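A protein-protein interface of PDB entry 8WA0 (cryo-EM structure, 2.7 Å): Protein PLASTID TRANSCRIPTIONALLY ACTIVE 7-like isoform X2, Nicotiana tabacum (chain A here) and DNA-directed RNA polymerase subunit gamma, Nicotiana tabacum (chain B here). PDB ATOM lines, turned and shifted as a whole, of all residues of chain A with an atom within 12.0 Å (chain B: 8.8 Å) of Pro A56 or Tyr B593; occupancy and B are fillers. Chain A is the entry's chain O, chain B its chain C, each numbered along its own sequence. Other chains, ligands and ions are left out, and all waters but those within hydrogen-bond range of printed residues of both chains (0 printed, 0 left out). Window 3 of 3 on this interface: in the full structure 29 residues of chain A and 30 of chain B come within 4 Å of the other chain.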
ATOM      1  N   ARG A  54      -5.802  27.637 -28.157  1.00  0.00           N
ATOM      2  CA  ARG A  54      -5.294  26.879 -27.024  1.00  0.00           C
ATOM      3  C   ARG A  54      -5.526  25.409 -27.272  1.00  0.00           C
ATOM      4  O   ARG A  54      -6.658  24.992 -27.480  1.00  0.00           O
ATOM      5  CB  ARG A  54      -6.012  27.293 -25.745  1.00  0.00           C
ATOM      6  CG  ARG A  54      -5.325  26.839 -24.473  1.00  0.00           C
ATOM      7  CD  ARG A  54      -4.045  27.626 -24.267  1.00  0.00           C
ATOM      8  NE  ARG A  54      -4.318  29.034 -24.009  1.00  0.00           N
ATOM      9  CZ  ARG A  54      -3.385  29.976 -23.945  1.00  0.00           C
ATOM     10  NH1 ARG A  54      -2.111  29.666 -24.134  1.00  0.00           N
ATOM     11  NH2 ARG A  54      -3.727  31.233 -23.704  1.00  0.00           N
ATOM     12  N   ILE A  55      -4.467  24.616 -27.255  1.00  0.00           N
ATOM     13  CA  ILE A  55      -4.649  23.190 -27.414  1.00  0.00           C
ATOM     14  C   ILE A  55      -5.447  22.710 -26.220  1.00  0.00           C
ATOM     15  O   ILE A  55      -5.227  23.152 -25.098  1.00  0.00           O
ATOM     16  CB  ILE A  55      -3.314  22.446 -27.619  1.00  0.00           C
ATOM     17  CG1 ILE A  55      -3.088  22.144 -29.100  1.00  0.00           C
ATOM     18  CG2 ILE A  55      -3.289  21.124 -26.872  1.00  0.00           C
ATOM     19  CD1 ILE A  55      -3.150  23.351 -30.008  1.00  0.00           C
ATOM     20  N   PRO A  56      -6.400  21.822 -26.461  1.00  0.00           N
ATOM     21  CA  PRO A  56      -7.279  21.390 -25.384  1.00  0.00           C
ATOM     22  C   PRO A  56      -6.738  20.653 -24.175  1.00  0.00           C
ATOM     23  O   PRO A  56      -7.169  20.983 -23.077  1.00  0.00           O
ATOM     24  CB  PRO A  56      -8.260  20.483 -26.112  1.00  0.00           C
ATOM     25  CG  PRO A  56      -8.342  21.053 -27.477  1.00  0.00           C
ATOM     26  CD  PRO A  56      -6.938  21.470 -27.784  1.00  0.00           C
ATOM     27  N   PHE A  57      -5.822  19.711 -24.313  1.00  0.00           N
ATOM     28  CA  PHE A  57      -5.441  18.938 -23.137  1.00  0.00           C
ATOM     29  C   PHE A  57      -3.969  18.903 -22.833  1.00  0.00           C
ATOM     30  O   PHE A  57      -3.332  17.876 -22.995  1.00  0.00           O
ATOM     31  CB  PHE A  57      -5.872  17.486 -23.299  1.00  0.00           C
ATOM     32  CG  PHE A  57      -7.148  17.291 -24.055  1.00  0.00           C
ATOM     33  CD1 PHE A  57      -8.370  17.462 -23.439  1.00  0.00           C
ATOM     34  CD2 PHE A  57      -7.122  16.884 -25.374  1.00  0.00           C
ATOM     35  CE1 PHE A  57      -9.542  17.265 -24.132  1.00  0.00           C
ATOM     36  CE2 PHE A  57      -8.290  16.684 -26.074  1.00  0.00           C
ATOM     37  CZ  PHE A  57      -9.500  16.872 -25.450  1.00  0.00           C
ATOM     38  N   LEU A  58      -3.425  20.007 -22.363  1.00  0.00           N
ATOM     39  CA  LEU A  58      -2.012  20.066 -22.092  1.00  0.00           C
ATOM     40  C   LEU A  58      -1.733  20.215 -20.624  1.00  0.00           C
ATOM     41  O   LEU A  58      -0.586  20.353 -20.231  1.00  0.00           O
ATOM     42  CB  LEU A  58      -1.433  21.245 -22.854  1.00  0.00           C
ATOM     43  CG  LEU A  58      -0.328  20.961 -23.862  1.00  0.00           C
ATOM     44  CD1 LEU A  58      -0.572  19.635 -24.557  1.00  0.00           C
ATOM     45  CD2 LEU A  58      -0.222  22.097 -24.864  1.00  0.00           C
ATOM     46  N   GLU A  59      -2.755  20.159 -19.795  1.00  0.00           N
ATOM     47  CA  GLU A  59      -2.580  20.420 -18.372  1.00  0.00           C
ATOM     48  C   GLU A  59      -1.513  19.645 -17.623  1.00  0.00           C
ATOM     49  O   GLU A  59      -0.758  20.234 -16.866  1.00  0.00           O
ATOM     50  CB  GLU A  59      -3.920  20.295 -17.664  1.00  0.00           C
ATOM     51  N   GLU A  60      -1.440  18.340 -17.813  1.00  0.00           N
ATOM     52  CA  GLU A  60      -0.489  17.517 -17.080  1.00  0.00           C
ATOM     53  C   GLU A  60       0.928  17.836 -17.442  1.00  0.00           C
ATOM     54  O   GLU A  60       1.768  17.946 -16.569  1.00  0.00           O
ATOM     55  CB  GLU A  60      -0.740  16.052 -17.353  1.00  0.00           C
ATOM     56  CG  GLU A  60      -0.913  15.197 -16.109  1.00  0.00           C
ATOM     57  CD  GLU A  60       0.256  15.304 -15.151  1.00  0.00           C
ATOM     58  OE1 GLU A  60       1.358  14.843 -15.511  1.00  0.00           O
ATOM     59  OE2 GLU A  60       0.074  15.849 -14.041  1.00  0.00           O
ATOM     60  N   GLN A  61       1.211  17.956 -18.725  1.00  0.00           N
ATOM     61  CA  GLN A  61       2.527  18.308 -19.190  1.00  0.00           C
ATOM     62  C   GLN A  61       2.997  19.614 -18.592  1.00  0.00           C
ATOM     63  O   GLN A  61       4.120  19.686 -18.122  1.00  0.00           O
ATOM     64  CB  GLN A  61       2.519  18.313 -20.699  1.00  0.00           C
ATOM     65  CG  GLN A  61       3.722  18.955 -21.346  1.00  0.00           C
ATOM     66  CD  GLN A  61       3.618  18.902 -22.845  1.00  0.00           C
ATOM     67  OE1 GLN A  61       3.022  17.986 -23.392  1.00  0.00           O
ATOM     68  NE2 GLN A  61       4.193  19.883 -23.517  1.00  0.00           N
ATOM     69  N   VAL A  62       2.156  20.628 -18.526  1.00  0.00           N
ATOM     70  CA  VAL A  62       2.537  21.856 -17.864  1.00  0.00           C
ATOM     71  C   VAL A  62       2.787  21.704 -16.369  1.00  0.00           C
ATOM     72  O   VAL A  62       3.727  22.283 -15.854  1.00  0.00           O
ATOM     73  CB  VAL A  62       1.649  23.027 -18.240  1.00  0.00           C
ATOM     74  CG1 VAL A  62       2.179  24.324 -17.673  1.00  0.00           C
ATOM     75  CG2 VAL A  62       1.544  23.134 -19.747  1.00  0.00           C
ATOM     76  N   ARG A  63       2.011  20.899 -15.662  1.00  0.00           N
ATOM     77  CA  ARG A  63       2.278  20.660 -14.249  1.00  0.00           C
ATOM     78  C   ARG A  63       3.578  20.011 -14.067  1.00  0.00           C
ATOM     79  O   ARG A  63       4.336  20.380 -13.180  1.00  0.00           O
ATOM     80  CB  ARG A  63       1.220  19.838 -13.574  1.00  0.00           C
ATOM     81  CG  ARG A  63       0.055  20.634 -13.048  1.00  0.00           C
ATOM     82  CD  ARG A  63      -0.822  19.740 -12.207  1.00  0.00           C
ATOM     83  NE  ARG A  63      -1.242  18.558 -12.943  1.00  0.00           N
ATOM     84  CZ  ARG A  63      -2.426  18.429 -13.522  1.00  0.00           C
ATOM     85  NH1 ARG A  63      -3.312  19.409 -13.445  1.00  0.00           N
ATOM     86  NH2 ARG A  63      -2.728  17.319 -14.171  1.00  0.00           N
ATOM     87  N   PHE B 589     -13.240  12.574 -40.535  1.00  0.00           N
ATOM     88  CA  PHE B 589     -13.168  13.148 -39.208  1.00  0.00           C
ATOM     89  C   PHE B 589     -12.902  14.625 -39.328  1.00  0.00           C
ATOM     90  O   PHE B 589     -12.208  15.047 -40.237  1.00  0.00           O
ATOM     91  CB  PHE B 589     -12.047  12.504 -38.426  1.00  0.00           C
ATOM     92  CG  PHE B 589     -12.308  11.087 -38.036  1.00  0.00           C
ATOM     93  CD1 PHE B 589     -13.181  10.792 -37.011  1.00  0.00           C
ATOM     94  CD2 PHE B 589     -11.659  10.052 -38.675  1.00  0.00           C
ATOM     95  CE1 PHE B 589     -13.418   9.487 -36.641  1.00  0.00           C
ATOM     96  CE2 PHE B 589     -11.889   8.746 -38.309  1.00  0.00           C
ATOM     97  CZ  PHE B 589     -12.770   8.461 -37.292  1.00  0.00           C
ATOM     98  N   SER B 590     -13.437  15.422 -38.416  1.00  0.00           N
ATOM     99  CA  SER B 590     -13.296  16.872 -38.516  1.00  0.00           C
ATOM    100  C   SER B 590     -12.129  17.468 -37.759  1.00  0.00           C
ATOM    101  O   SER B 590     -11.589  18.485 -38.160  1.00  0.00           O
ATOM    102  CB  SER B 590     -14.568  17.531 -38.028  1.00  0.00           C
ATOM    103  OG  SER B 590     -15.700  16.949 -38.643  1.00  0.00           O
ATOM    104  N   ASN B 591     -11.751  16.862 -36.653  1.00  0.00           N
ATOM    105  CA  ASN B 591     -10.649  17.340 -35.883  1.00  0.00           C
ATOM    106  C   ASN B 591      -9.812  16.149 -35.570  1.00  0.00           C
ATOM    107  O   ASN B 591     -10.292  15.039 -35.601  1.00  0.00           O
ATOM    108  CB  ASN B 591     -11.153  17.893 -34.574  1.00  0.00           C
ATOM    109  CG  ASN B 591     -11.654  19.314 -34.693  1.00  0.00           C
ATOM    110  OD1 ASN B 591     -12.497  19.750 -33.911  1.00  0.00           O
ATOM    111  ND2 ASN B 591     -11.138  20.048 -35.672  1.00  0.00           N
ATOM    112  N   SER B 592      -8.547  16.366 -35.259  1.00  0.00           N
ATOM    113  CA  SER B 592      -7.650  15.258 -35.024  1.00  0.00           C
ATOM    114  C   SER B 592      -7.959  14.532 -33.748  1.00  0.00           C
ATOM    115  O   SER B 592      -7.663  13.359 -33.616  1.00  0.00           O
ATOM    116  CB  SER B 592      -6.221  15.754 -34.990  1.00  0.00           C
ATOM    117  OG  SER B 592      -6.071  16.771 -34.022  1.00  0.00           O
ATOM    118  N   TYR B 593      -8.543  15.218 -32.789  1.00  0.00           N
ATOM    119  CA  TYR B 593      -8.801  14.601 -31.500  1.00  0.00           C
ATOM    120  C   TYR B 593      -9.780  13.472 -31.628  1.00  0.00           C
ATOM    121  O   TYR B 593      -9.635  12.444 -30.986  1.00  0.00           O
ATOM    122  CB  TYR B 593      -9.271  15.642 -30.501  1.00  0.00           C
ATOM    123  CG  TYR B 593      -8.361  16.837 -30.495  1.00  0.00           C
ATOM    124  CD1 TYR B 593      -7.072  16.742 -29.997  1.00  0.00           C
ATOM    125  CD2 TYR B 593      -8.775  18.050 -31.016  1.00  0.00           C
ATOM    126  CE1 TYR B 593      -6.223  17.827 -30.006  1.00  0.00           C
ATOM    127  CE2 TYR B 593      -7.934  19.141 -31.028  1.00  0.00           C
ATOM    128  CZ  TYR B 593      -6.661  19.022 -30.523  1.00  0.00           C
ATOM    129  OH  TYR B 593      -5.822  20.107 -30.535  1.00  0.00           O
ATOM    130  N   ASP B 594     -10.782  13.661 -32.462  1.00  0.00           N
ATOM    131  CA  ASP B 594     -11.786  12.644 -32.630  1.00  0.00           C
ATOM    132  C   ASP B 594     -11.153  11.385 -33.147  1.00  0.00           C
ATOM    133  O   ASP B 594     -11.496  10.296 -32.714  1.00  0.00           O
ATOM    134  CB  ASP B 594     -12.808  13.130 -33.633  1.00  0.00           C
ATOM    135  CG  ASP B 594     -13.293  14.528 -33.336  1.00  0.00           C
ATOM    136  OD1 ASP B 594     -13.289  14.920 -32.152  1.00  0.00           O
ATOM    137  OD2 ASP B 594     -13.687  15.234 -34.286  1.00  0.00           O
ATOM    138  N   ALA B 595     -10.230  11.524 -34.077  1.00  0.00           N
ATOM    139  CA  ALA B 595      -9.596  10.385 -34.672  1.00  0.00           C
ATOM    140  C   ALA B 595      -8.815   9.587 -33.715  1.00  0.00           C
ATOM    141  O   ALA B 595      -8.883   8.360 -33.724  1.00  0.00           O
ATOM    142  CB  ALA B 595      -8.692  10.839 -35.761  1.00  0.00           C
ATOM    143  N   ILE B 596      -8.065  10.257 -32.865  1.00  0.00           N
ATOM    144  CA  ILE B 596      -7.260   9.581 -31.883  1.00  0.00           C
ATOM    145  C   ILE B 596      -8.194   8.852 -30.965  1.00  0.00           C
ATOM    146  O   ILE B 596      -7.914   7.738 -30.548  1.00  0.00           O
ATOM    147  CB  ILE B 596      -6.246  10.527 -31.263  1.00  0.00           C
ATOM    148  CG1 ILE B 596      -5.270  10.993 -32.329  1.00  0.00           C
ATOM    149  CG2 ILE B 596      -5.477   9.847 -30.146  1.00  0.00           C
ATOM    150  CD1 ILE B 596      -3.901  11.317 -31.792  1.00  0.00           C
ATOM    151  N   GLY B 597      -9.328   9.436 -30.678  1.00  0.00           N
ATOM    152  CA  GLY B 597     -10.321   8.804 -29.861  1.00  0.00           C
ATOM    153  C   GLY B 597     -10.897   7.537 -30.403  1.00  0.00           C
ATOM    154  O   GLY B 597     -11.152   6.617 -29.647  1.00  0.00           O
ATOM    155  N   ALA B 598     -11.110   7.471 -31.701  1.00  0.00           N
ATOM    156  CA  ALA B 598     -11.724   6.300 -32.267  1.00  0.00           C
ATOM    157  C   ALA B 598     -10.778   5.147 -32.145  1.00  0.00           C
ATOM    158  O   ALA B 598     -11.199   4.011 -32.016  1.00  0.00           O
ATOM    159  CB  ALA B 598     -12.060   6.538 -33.705  1.00  0.00           C
ATOM    160  N   TYR B 599      -9.490   5.433 -32.185  1.00  0.00           N
ATOM    161  CA  TYR B 599      -8.505   4.381 -32.094  1.00  0.00           C
ATOM    162  C   TYR B 599      -8.629   3.726 -30.753  1.00  0.00           C
ATOM    163  O   TYR B 599      -8.524   2.514 -30.638  1.00  0.00           O
ATOM    164  CB  TYR B 599      -7.103   4.933 -32.275  1.00  0.00           C
ATOM    165  CG  TYR B 599      -6.019   3.894 -32.284  1.00  0.00           C
ATOM    166  CD1 TYR B 599      -6.108   2.780 -33.099  1.00  0.00           C
ATOM    167  CD2 TYR B 599      -4.898   4.036 -31.489  1.00  0.00           C
ATOM    168  CE1 TYR B 599      -5.115   1.827 -33.109  1.00  0.00           C
ATOM    169  CE2 TYR B 599      -3.895   3.089 -31.497  1.00  0.00           C
ATOM    170  CZ  TYR B 599      -4.009   1.987 -32.309  1.00  0.00           C
ATOM    171  OH  TYR B 599      -3.011   1.040 -32.318  1.00  0.00           O
ATOM    172  N   ARG B 600      -8.853   4.521 -29.725  1.00  0.00           N
ATOM    173  CA  ARG B 600      -8.952   3.978 -28.392  1.00  0.00           C
ATOM    174  C   ARG B 600     -10.213   3.160 -28.230  1.00  0.00           C
ATOM    175  O   ARG B 600     -10.185   2.077 -27.659  1.00  0.00           O
ATOM    176  CB  ARG B 600      -8.929   5.109 -27.379  1.00  0.00           C
ATOM    177  CG  ARG B 600      -7.714   6.011 -27.510  1.00  0.00           C
ATOM    178  CD  ARG B 600      -7.646   7.052 -26.403  1.00  0.00           C
ATOM    179  NE  ARG B 600      -8.559   8.176 -26.602  1.00  0.00           N
ATOM    180  CZ  ARG B 600      -9.745   8.297 -26.014  1.00  0.00           C
ATOM    181  NH1 ARG B 600     -10.175   7.360 -25.184  1.00  0.00           N
ATOM    182  NH2 ARG B 600     -10.502   9.358 -26.253  1.00  0.00           N
ATOM    183  N   ILE B 604     -11.550   2.157 -35.094  1.00  0.00           N
ATOM    184  CA  ILE B 604     -10.652   1.969 -36.235  1.00  0.00           C
ATOM    185  C   ILE B 604      -9.332   1.343 -35.804  1.00  0.00           C
ATOM    186  O   ILE B 604      -9.053   1.245 -34.608  1.00  0.00           O
ATOM    187  CB  ILE B 604     -10.345   3.303 -36.947  1.00  0.00           C
ATOM    188  CG1 ILE B 604      -9.779   4.322 -35.956  1.00  0.00           C
ATOM    189  CG2 ILE B 604     -11.586   3.857 -37.630  1.00  0.00           C
ATOM    190  CD1 ILE B 604      -9.529   5.685 -36.558  1.00  0.00           C
ATOM    191  N   LEU B 612      -9.150  13.571 -43.087  1.00  0.00           N
ATOM    192  CA  LEU B 612      -9.144  14.594 -42.055  1.00  0.00           C
ATOM    193  C   LEU B 612      -9.235  15.960 -42.662  1.00  0.00           C
ATOM    194  O   LEU B 612      -8.511  16.260 -43.588  1.00  0.00           O
ATOM    195  CB  LEU B 612      -7.855  14.516 -41.253  1.00  0.00           C
ATOM    196  CG  LEU B 612      -7.686  15.418 -40.040  1.00  0.00           C
ATOM    197  CD1 LEU B 612      -8.645  14.984 -38.950  1.00  0.00           C
ATOM    198  CD2 LEU B 612      -6.252  15.333 -39.554  1.00  0.00           C
ATOM    199  N   ILE B 667      -1.062  11.044 -37.535  1.00  0.00           N
ATOM    200  CA  ILE B 667      -1.545  12.177 -36.779  1.00  0.00           C
ATOM    201  C   ILE B 667      -1.002  12.184 -35.370  1.00  0.00           C
ATOM    202  O   ILE B 667      -0.764  13.245 -34.825  1.00  0.00           O
ATOM    203  CB  ILE B 667      -3.073  12.314 -36.834  1.00  0.00           C
ATOM    204  CG1 ILE B 667      -3.767  11.424 -35.827  1.00  0.00           C
ATOM    205  CG2 ILE B 667      -3.583  12.007 -38.230  1.00  0.00           C
ATOM    206  CD1 ILE B 667      -5.222  11.245 -36.161  1.00  0.00           C
ATOM    207  N   ARG B 671       0.931  15.445 -33.562  1.00  0.00           N
ATOM    208  CA  ARG B 671       0.403  15.983 -32.368  1.00  0.00           C
ATOM    209  C   ARG B 671       1.377  16.029 -31.213  1.00  0.00           C
ATOM    210  O   ARG B 671       1.435  17.040 -30.545  1.00  0.00           O
ATOM    211  CB  ARG B 671      -0.879  15.274 -32.044  1.00  0.00           C
ATOM    212  CG  ARG B 671      -1.533  15.650 -30.731  1.00  0.00           C
ATOM    213  CD  ARG B 671      -2.802  14.841 -30.537  1.00  0.00           C
ATOM    214  NE  ARG B 671      -3.346  14.986 -29.192  1.00  0.00           N
ATOM    215  CZ  ARG B 671      -4.458  14.394 -28.772  1.00  0.00           C
ATOM    216  NH1 ARG B 671      -5.151  13.618 -29.597  1.00  0.00           N
ATOM    217  NH2 ARG B 671      -4.880  14.577 -27.531  1.00  0.00           N
ATOM    218  N   GLU B 674       3.904  18.898 -31.811  1.00  0.00           N
ATOM    219  CA  GLU B 674       3.260  20.177 -31.653  1.00  0.00           C
ATOM    220  C   GLU B 674       2.912  20.545 -30.251  1.00  0.00           C
ATOM    221  O   GLU B 674       3.149  21.662 -29.828  1.00  0.00           O
ATOM    222  CB  GLU B 674       2.050  20.276 -32.575  1.00  0.00           C
ATOM    223  CG  GLU B 674       1.838  21.634 -33.216  1.00  0.00           C
ATOM    224  CD  GLU B 674       1.117  22.615 -32.312  1.00  0.00           C
ATOM    225  OE1 GLU B 674       1.335  23.835 -32.466  1.00  0.00           O
ATOM    226  OE2 GLU B 674       0.336  22.170 -31.444  1.00  0.00           O
ATOM    227  N   GLU B 675       2.375  19.633 -29.504  1.00  0.00           N
ATOM    228  CA  GLU B 675       2.022  19.861 -28.145  1.00  0.00           C
ATOM    229  C   GLU B 675       3.178  20.120 -27.238  1.00  0.00           C
ATOM    230  O   GLU B 675       3.063  20.908 -26.326  1.00  0.00           O
ATOM    231  CB  GLU B 675       1.137  18.734 -27.689  1.00  0.00           C
ATOM    232  CG  GLU B 675       1.838  17.442 -27.310  1.00  0.00           C
ATOM    233  CD  GLU B 675       0.865  16.316 -27.032  1.00  0.00           C
ATOM    234  OE1 GLU B 675      -0.357  16.543 -27.156  1.00  0.00           O
ATOM    235  OE2 GLU B 675       1.321  15.205 -26.693  1.00  0.00           O
ATOM    236  N   GLN B 678       4.174  23.791 -27.678  1.00  0.00           N
ATOM    237  CA  GLN B 678       3.245  24.710 -27.064  1.00  0.00           C
ATOM    238  C   GLN B 678       3.286  24.621 -25.566  1.00  0.00           C
ATOM    239  O   GLN B 678       3.158  25.618 -24.880  1.00  0.00           O
ATOM    240  CB  GLN B 678       1.850  24.432 -27.578  1.00  0.00           C
ATOM    241  CG  GLN B 678       0.810  25.462 -27.191  1.00  0.00           C
ATOM    242  CD  GLN B 678      -0.387  25.425 -28.112  1.00  0.00           C
ATOM    243  OE1 GLN B 678      -0.299  24.931 -29.234  1.00  0.00           O
ATOM    244  NE2 GLN B 678      -1.513  25.955 -27.647  1.00  0.00           N
ATOM    245  N   ARG B 682       3.959  27.610 -22.761  1.00  0.00           N
ATOM    246  CA  ARG B 682       2.999  28.033 -21.767  1.00  0.00           C
ATOM    247  C   ARG B 682       3.551  27.894 -20.386  1.00  0.00           C
ATOM    248  O   ARG B 682       3.094  28.561 -19.477  1.00  0.00           O
ATOM    249  CB  ARG B 682       1.694  27.266 -21.894  1.00  0.00           C
ATOM    250  CG  ARG B 682       0.768  27.803 -22.969  1.00  0.00           C
ATOM    251  CD  ARG B 682      -0.293  26.786 -23.345  1.00  0.00           C
ATOM    252  NE  ARG B 682      -0.977  26.239 -22.179  1.00  0.00           N
ATOM    253  CZ  ARG B 682      -1.923  25.308 -22.242  1.00  0.00           C
ATOM    254  NH1 ARG B 682      -2.300  24.823 -23.416  1.00  0.00           N
ATOM    255  NH2 ARG B 682      -2.491  24.860 -21.134  1.00  0.00           N
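Of chain B, only Tyr B593, Glu B674, Gln B678 and Arg B682 come within 4 Å of Ile A55. Printed residues of chain B within 4 Å of Pro A56: Tyr B593. Of chain B, only Arg B671 (3.9 Å) comes within 4 Å of Phe A57. Of the printed residues of chain B, Leu A58 touches Glu B675 (3.7 Å) and Arg B682 (3.7 Å). Of the printed residues of chain B, Gln A61 touches Glu B675 (3.2 Å). No residue of chain A comes within 4 Å of Asn B591. No residue of chain A comes within 4 Å of Ser B592. Of chain A, only Ile A55 and Pro A56 come within 4 Å of Tyr B593. No residue of chain A comes within 4 Å of Asp B594. No residue of chain A comes within 4 Å of Ala B595. Gly B597 touches none of the printed residues of chain A. Leu B612 touches none of the printed residues of chain A. Of the printed residues of chain A, Glu B675 touches Leu A58 (3.7 Å) and Gln A61 (3.2 Å). Printed residues of chain A within 4 Å of Gln B678: Arg A54 and Ile A55. Of the printed residues of chain A, Arg B682 touches Arg A54 (3.4 Å), Ile A55 (3.8 Å) and Leu A58 (3.7 Å). The nearest residue of chain A that does not touch Tyr B593 is Phe A57 (4.1 Å).
The backbone NH (N) of Ile A55 sits close to the side-chain amide nitrogen (NE2) of Gln B678 (3.3 Å). The side-chain amide nitrogen (NE2) of Gln A61 sits at hydrogen-bond distance from the backbone carbonyl oxygen (O) of Glu B675 (3.2 Å).
The guanidinium group (NE) of Arg B671 lies within salt-bridge range of the side-chain carboxylate (OE1) of Glu B675, at 3.9 Å.
Among the printed residues, merely in contact across the chains: Pro A56 with Tyr B593, Arg A54 with Arg B682, Leu A58 with Glu B675, Ile A55 with Tyr B593, Leu A58 with Arg B682, Ile A55 with Arg B682, Phe A57 with Arg B671, Arg A54 with Gln B678 and Ile A55 with Glu B674.
Printed residues of chain B that touch a printed residue of chain A: Tyr B593, Arg B671, Glu B674, Glu B675, Gln B678 and Arg B682. Hydrophobic or aromatic side chains of chain A within 4 Å of the printed part of chain B: Ile A55, Pro A56, Phe A57 and Leu A58.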
